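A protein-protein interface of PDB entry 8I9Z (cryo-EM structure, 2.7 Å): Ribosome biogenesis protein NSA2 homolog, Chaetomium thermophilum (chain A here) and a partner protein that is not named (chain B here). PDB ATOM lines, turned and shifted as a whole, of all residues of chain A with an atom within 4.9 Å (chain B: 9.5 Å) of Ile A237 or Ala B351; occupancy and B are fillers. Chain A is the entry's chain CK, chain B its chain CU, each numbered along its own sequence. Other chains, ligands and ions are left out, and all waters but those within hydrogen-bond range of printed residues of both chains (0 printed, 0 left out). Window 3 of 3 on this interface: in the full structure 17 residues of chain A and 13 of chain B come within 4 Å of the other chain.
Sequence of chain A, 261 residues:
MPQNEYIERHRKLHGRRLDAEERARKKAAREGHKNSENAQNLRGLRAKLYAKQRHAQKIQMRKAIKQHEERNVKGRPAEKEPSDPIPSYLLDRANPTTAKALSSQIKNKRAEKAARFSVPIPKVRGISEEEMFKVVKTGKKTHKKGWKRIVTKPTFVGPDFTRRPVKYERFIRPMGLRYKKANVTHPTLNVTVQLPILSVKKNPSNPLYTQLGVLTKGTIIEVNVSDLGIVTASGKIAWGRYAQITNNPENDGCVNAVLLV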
ATOM      1  N   SER A 226      -4.673  -5.922  -2.625  1.00  0.00           N
ATOM      2  CA  SER A 226      -3.267  -5.723  -2.952  1.00  0.00           C
ATOM      3  C   SER A 226      -2.830  -4.284  -2.722  1.00  0.00           C
ATOM      4  O   SER A 226      -1.687  -4.040  -2.322  1.00  0.00           O
ATOM      5  CB  SER A 226      -3.005  -6.131  -4.399  1.00  0.00           C
ATOM      6  OG  SER A 226      -3.665  -5.263  -5.299  1.00  0.00           O
ATOM      7  N   GLY A 229      -2.076  -3.140   1.207  1.00  0.00           N
ATOM      8  CA  GLY A 229      -0.810  -3.475   1.829  1.00  0.00           C
ATOM      9  C   GLY A 229      -0.926  -4.118   3.193  1.00  0.00           C
ATOM     10  O   GLY A 229      -0.178  -3.773   4.110  1.00  0.00           O
ATOM     11  N   ILE A 230      -1.858  -5.052   3.344  1.00  0.00           N
ATOM     12  CA  ILE A 230      -2.028  -5.756   4.609  1.00  0.00           C
ATOM     13  C   ILE A 230      -0.914  -6.780   4.744  1.00  0.00           C
ATOM     14  O   ILE A 230      -0.743  -7.645   3.879  1.00  0.00           O
ATOM     15  CB  ILE A 230      -3.404  -6.428   4.694  1.00  0.00           C
ATOM     16  CG1 ILE A 230      -4.490  -5.496   4.164  1.00  0.00           C
ATOM     17  CG2 ILE A 230      -3.698  -6.844   6.123  1.00  0.00           C
ATOM     18  CD1 ILE A 230      -5.879  -6.066   4.256  1.00  0.00           C
ATOM     19  N   VAL A 231      -0.155  -6.690   5.830  1.00  0.00           N
ATOM     20  CA  VAL A 231       0.930  -7.620   6.112  1.00  0.00           C
ATOM     21  C   VAL A 231       0.357  -8.693   7.028  1.00  0.00           C
ATOM     22  O   VAL A 231       0.004  -8.422   8.179  1.00  0.00           O
ATOM     23  CB  VAL A 231       2.134  -6.921   6.743  1.00  0.00           C
ATOM     24  CG1 VAL A 231       3.160  -7.948   7.195  1.00  0.00           C
ATOM     25  CG2 VAL A 231       2.747  -5.934   5.768  1.00  0.00           C
ATOM     26  N   THR A 232       0.257  -9.912   6.517  1.00  0.00           N
ATOM     27  CA  THR A 232      -0.276 -11.010   7.301  1.00  0.00           C
ATOM     28  C   THR A 232       0.829 -11.616   8.160  1.00  0.00           C
ATOM     29  O   THR A 232       1.949 -11.104   8.240  1.00  0.00           O
ATOM     30  CB  THR A 232      -0.889 -12.065   6.387  1.00  0.00           C
ATOM     31  OG1 THR A 232       0.122 -12.589   5.520  1.00  0.00           O
ATOM     32  CG2 THR A 232      -1.998 -11.456   5.544  1.00  0.00           C
ATOM     33  N   GLY A 235       4.727 -12.523   7.004  1.00  0.00           N
ATOM     34  CA  GLY A 235       5.211 -11.433   6.169  1.00  0.00           C
ATOM     35  C   GLY A 235       4.754 -11.456   4.728  1.00  0.00           C
ATOM     36  O   GLY A 235       5.530 -11.115   3.827  1.00  0.00           O
ATOM     37  N   LYS A 236       3.509 -11.839   4.488  1.00  0.00           N
ATOM     38  CA  LYS A 236       2.967 -11.930   3.143  1.00  0.00           C
ATOM     39  C   LYS A 236       1.907 -10.857   2.946  1.00  0.00           C
ATOM     40  O   LYS A 236       1.063 -10.639   3.819  1.00  0.00           O
ATOM     41  CB  LYS A 236       2.367 -13.313   2.890  1.00  0.00           C
ATOM     42  CG  LYS A 236       3.335 -14.294   2.268  1.00  0.00           C
ATOM     43  CD  LYS A 236       3.146 -15.689   2.822  1.00  0.00           C
ATOM     44  CE  LYS A 236       3.987 -16.693   2.053  1.00  0.00           C
ATOM     45  NZ  LYS A 236       4.034 -16.368   0.606  1.00  0.00           N
ATOM     46  N   ILE A 237       1.960 -10.182   1.804  1.00  0.00           N
ATOM     47  CA  ILE A 237       0.956  -9.179   1.475  1.00  0.00           C
ATOM     48  C   ILE A 237      -0.321  -9.902   1.080  1.00  0.00           C
ATOM     49  O   ILE A 237      -0.310 -10.756   0.189  1.00  0.00           O
ATOM     50  CB  ILE A 237       1.439  -8.247   0.356  1.00  0.00           C
ATOM     51  CG1 ILE A 237       2.704  -7.491   0.772  1.00  0.00           C
ATOM     52  CG2 ILE A 237       0.344  -7.266  -0.030  1.00  0.00           C
ATOM     53  CD1 ILE A 237       2.677  -6.932   2.176  1.00  0.00           C
ATOM     54  N   ALA A 238      -1.418  -9.577   1.758  1.00  0.00           N
ATOM     55  CA  ALA A 238      -2.695 -10.203   1.466  1.00  0.00           C
ATOM     56  C   ALA A 238      -3.205  -9.766   0.101  1.00  0.00           C
ATOM     57  O   ALA A 238      -3.009  -8.626  -0.328  1.00  0.00           O
ATOM     58  CB  ALA A 238      -3.718  -9.853   2.543  1.00  0.00           C
ATOM     59  N   TRP A 239      -3.866 -10.691  -0.588  1.00  0.00           N
ATOM     60  CA  TRP A 239      -4.367 -10.437  -1.931  1.00  0.00           C
ATOM     61  C   TRP A 239      -5.848 -10.716  -2.117  1.00  0.00           C
ATOM     62  O   TRP A 239      -6.427 -10.213  -3.086  1.00  0.00           O
ATOM     63  CB  TRP A 239      -3.576 -11.252  -2.960  1.00  0.00           C
ATOM     64  CG  TRP A 239      -2.362 -10.545  -3.429  1.00  0.00           C
ATOM     65  CD1 TRP A 239      -1.212 -10.341  -2.733  1.00  0.00           C
ATOM     66  CD2 TRP A 239      -2.168  -9.949  -4.711  1.00  0.00           C
ATOM     67  NE1 TRP A 239      -0.314  -9.643  -3.499  1.00  0.00           N
ATOM     68  CE2 TRP A 239      -0.879  -9.391  -4.720  1.00  0.00           C
ATOM     69  CE3 TRP A 239      -2.963  -9.828  -5.850  1.00  0.00           C
ATOM     70  CZ2 TRP A 239      -0.365  -8.722  -5.825  1.00  0.00           C
ATOM     71  CZ3 TRP A 239      -2.453  -9.166  -6.945  1.00  0.00           C
ATOM     72  CH2 TRP A 239      -1.166  -8.622  -6.926  1.00  0.00           C
ATOM     73  N   GLY A 240      -6.481 -11.488  -1.244  1.00  0.00           N
ATOM     74  CA  GLY A 240      -7.906 -11.704  -1.337  1.00  0.00           C
ATOM     75  C   GLY A 240      -8.536 -11.843   0.027  1.00  0.00           C
ATOM     76  O   GLY A 240      -8.118 -12.692   0.818  1.00  0.00           O
ATOM     77  N   ARG A 241      -9.551 -11.034   0.314  1.00  0.00           N
ATOM     78  CA  ARG A 241     -10.164 -11.016   1.632  1.00  0.00           C
ATOM     79  C   ARG A 241     -11.680 -11.022   1.506  1.00  0.00           C
ATOM     80  O   ARG A 241     -12.247 -10.593   0.500  1.00  0.00           O
ATOM     81  CB  ARG A 241      -9.718  -9.799   2.443  1.00  0.00           C
ATOM     82  CG  ARG A 241      -9.013 -10.140   3.734  1.00  0.00           C
ATOM     83  CD  ARG A 241      -7.743 -10.885   3.452  1.00  0.00           C
ATOM     84  NE  ARG A 241      -7.009 -11.213   4.664  1.00  0.00           N
ATOM     85  CZ  ARG A 241      -5.946 -12.002   4.695  1.00  0.00           C
ATOM     86  NH1 ARG A 241      -5.483 -12.579   3.600  1.00  0.00           N
ATOM     87  NH2 ARG A 241      -5.331 -12.214   5.853  1.00  0.00           N
ATOM     88  N   ALA B 348      -3.336 -14.280  10.894  1.00  0.00           N
ATOM     89  CA  ALA B 348      -3.388 -15.722  11.092  1.00  0.00           C
ATOM     90  C   ALA B 348      -3.950 -16.423   9.863  1.00  0.00           C
ATOM     91  O   ALA B 348      -4.399 -17.563   9.938  1.00  0.00           O
ATOM     92  CB  ALA B 348      -4.218 -16.057  12.317  1.00  0.00           C
ATOM     93  N   LEU B 349      -3.920 -15.731   8.732  1.00  0.00           N
ATOM     94  CA  LEU B 349      -4.451 -16.225   7.471  1.00  0.00           C
ATOM     95  C   LEU B 349      -3.350 -16.219   6.416  1.00  0.00           C
ATOM     96  O   LEU B 349      -2.225 -15.778   6.659  1.00  0.00           O
ATOM     97  CB  LEU B 349      -5.641 -15.379   7.011  1.00  0.00           C
ATOM     98  CG  LEU B 349      -7.028 -15.718   7.551  1.00  0.00           C
ATOM     99  CD1 LEU B 349      -7.249 -15.088   8.915  1.00  0.00           C
ATOM    100  CD2 LEU B 349      -8.092 -15.255   6.572  1.00  0.00           C
ATOM    101  N   GLY B 350      -3.690 -16.712   5.229  1.00  0.00           N
ATOM    102  CA  GLY B 350      -2.772 -16.741   4.113  1.00  0.00           C
ATOM    103  C   GLY B 350      -2.852 -15.483   3.274  1.00  0.00           C
ATOM    104  O   GLY B 350      -3.495 -14.494   3.630  1.00  0.00           O
ATOM    105  N   ALA B 351      -2.167 -15.529   2.129  1.00  0.00           N
ATOM    106  CA  ALA B 351      -2.222 -14.416   1.191  1.00  0.00           C
ATOM    107  C   ALA B 351      -3.593 -14.301   0.541  1.00  0.00           C
ATOM    108  O   ALA B 351      -4.054 -13.189   0.263  1.00  0.00           O
ATOM    109  CB  ALA B 351      -1.141 -14.572   0.125  1.00  0.00           C
ATOM    110  N   THR B 352      -4.256 -15.427   0.301  1.00  0.00           N
ATOM    111  CA  THR B 352      -5.579 -15.437  -0.297  1.00  0.00           C
ATOM    112  C   THR B 352      -6.494 -16.312   0.545  1.00  0.00           C
ATOM    113  O   THR B 352      -6.047 -17.057   1.420  1.00  0.00           O
ATOM    114  CB  THR B 352      -5.546 -15.936  -1.747  1.00  0.00           C
ATOM    115  OG1 THR B 352      -6.835 -15.757  -2.342  1.00  0.00           O
ATOM    116  CG2 THR B 352      -5.171 -17.405  -1.797  1.00  0.00           C
ATOM    117  N   GLU B 353      -7.791 -16.201   0.279  1.00  0.00           N
ATOM    118  CA  GLU B 353      -8.779 -16.972   1.017  1.00  0.00           C
ATOM    119  C   GLU B 353      -8.719 -18.440   0.613  1.00  0.00           C
ATOM    120  O   GLU B 353      -8.195 -18.795  -0.446  1.00  0.00           O
ATOM    121  CB  GLU B 353     -10.179 -16.412   0.767  1.00  0.00           C
ATOM    122  CG  GLU B 353     -10.656 -15.329   1.745  1.00  0.00           C
ATOM    123  CD  GLU B 353     -10.582 -15.699   3.226  1.00  0.00           C
ATOM    124  OE1 GLU B 353     -10.588 -14.761   4.051  1.00  0.00           O
ATOM    125  OE2 GLU B 353     -10.598 -16.897   3.584  1.00  0.00           O
ATOM    126  N   ALA B 354      -9.253 -19.298   1.479  1.00  0.00           N
ATOM    127  CA  ALA B 354      -9.177 -20.735   1.262  1.00  0.00           C
ATOM    128  C   ALA B 354     -10.049 -21.160   0.087  1.00  0.00           C
ATOM    129  O   ALA B 354     -11.099 -20.568  -0.175  1.00  0.00           O
ATOM    130  CB  ALA B 354      -9.598 -21.482   2.526  1.00  0.00           C
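N of Trp A239 is in hydrogen-bond range of O of Ala B351, at 2.6 Å. The backbone NH of Gly A240 sits at hydrogen-bond distance from the backbone carbonyl oxygen of Ala B351, 3.3 Å away. O of Gly B350 is in hydrogen-bond range of NH1 of Arg A241, at 2.8 Å.
O of Ile A230 sits at hydrogen-bond distance from N of Ala A238, 2.9 Å away. The backbone carbonyl oxygen of Lys A236 lies within hydrogen-bond range of the side-chain hydroxyl of Thr A232 (2.8 Å).
Thr A232 touches Leu B349. Gly B350 touches Thr A232. Ala B351 touches Ile A237 (CB to O, 3.9 Å). Ala A238 touches Ala B351 (CA to O, 3.5 Å). Gly A240 touches Thr B352. Gly A240 touches Glu B353. NH2 of Arg A241 touches CB of Leu B349, 3.4 Å away. Ala B351 touches Arg A241 (O to NH1, 3.7 Å).
No residue of chain B comes within 4 Å of Gly A229. Ile A237 touches just one residue of chain B: Ala B351. Of chain B, only Ala B351 comes within 4 Å of Ala A238. Of the printed residues of chain B, Trp A239 touches Ala B351 (2.6 Å). Gly A240 touches three residues of chain B. Of the printed residues of chain B, Arg A241 touches Leu B349, Gly B350 and Ala B351. Of the printed residues of chain A, Ala B351 touches Ile A237, Ala A238, Trp A239, Gly A240 and Arg A241. Ala B354 touches none of the printed residues of chain A. The nearest residue of chain B that does not touch Ile A237 is Gly B350 (6.0 Å).
Hydrophobic or aromatic side chains of chain A within 4 Å of the printed part of chain B: Trp A239. Printed residues of chain B that touch a printed residue of chain A: Leu B349, Gly B350, Ala B351, Thr B352 and Glu B353. Hydrophobic or aromatic side chains of chain B that line the printed part of chain A: Leu B349 and Ala B351. Among the printed residues, 11 pairs touch across the chains.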
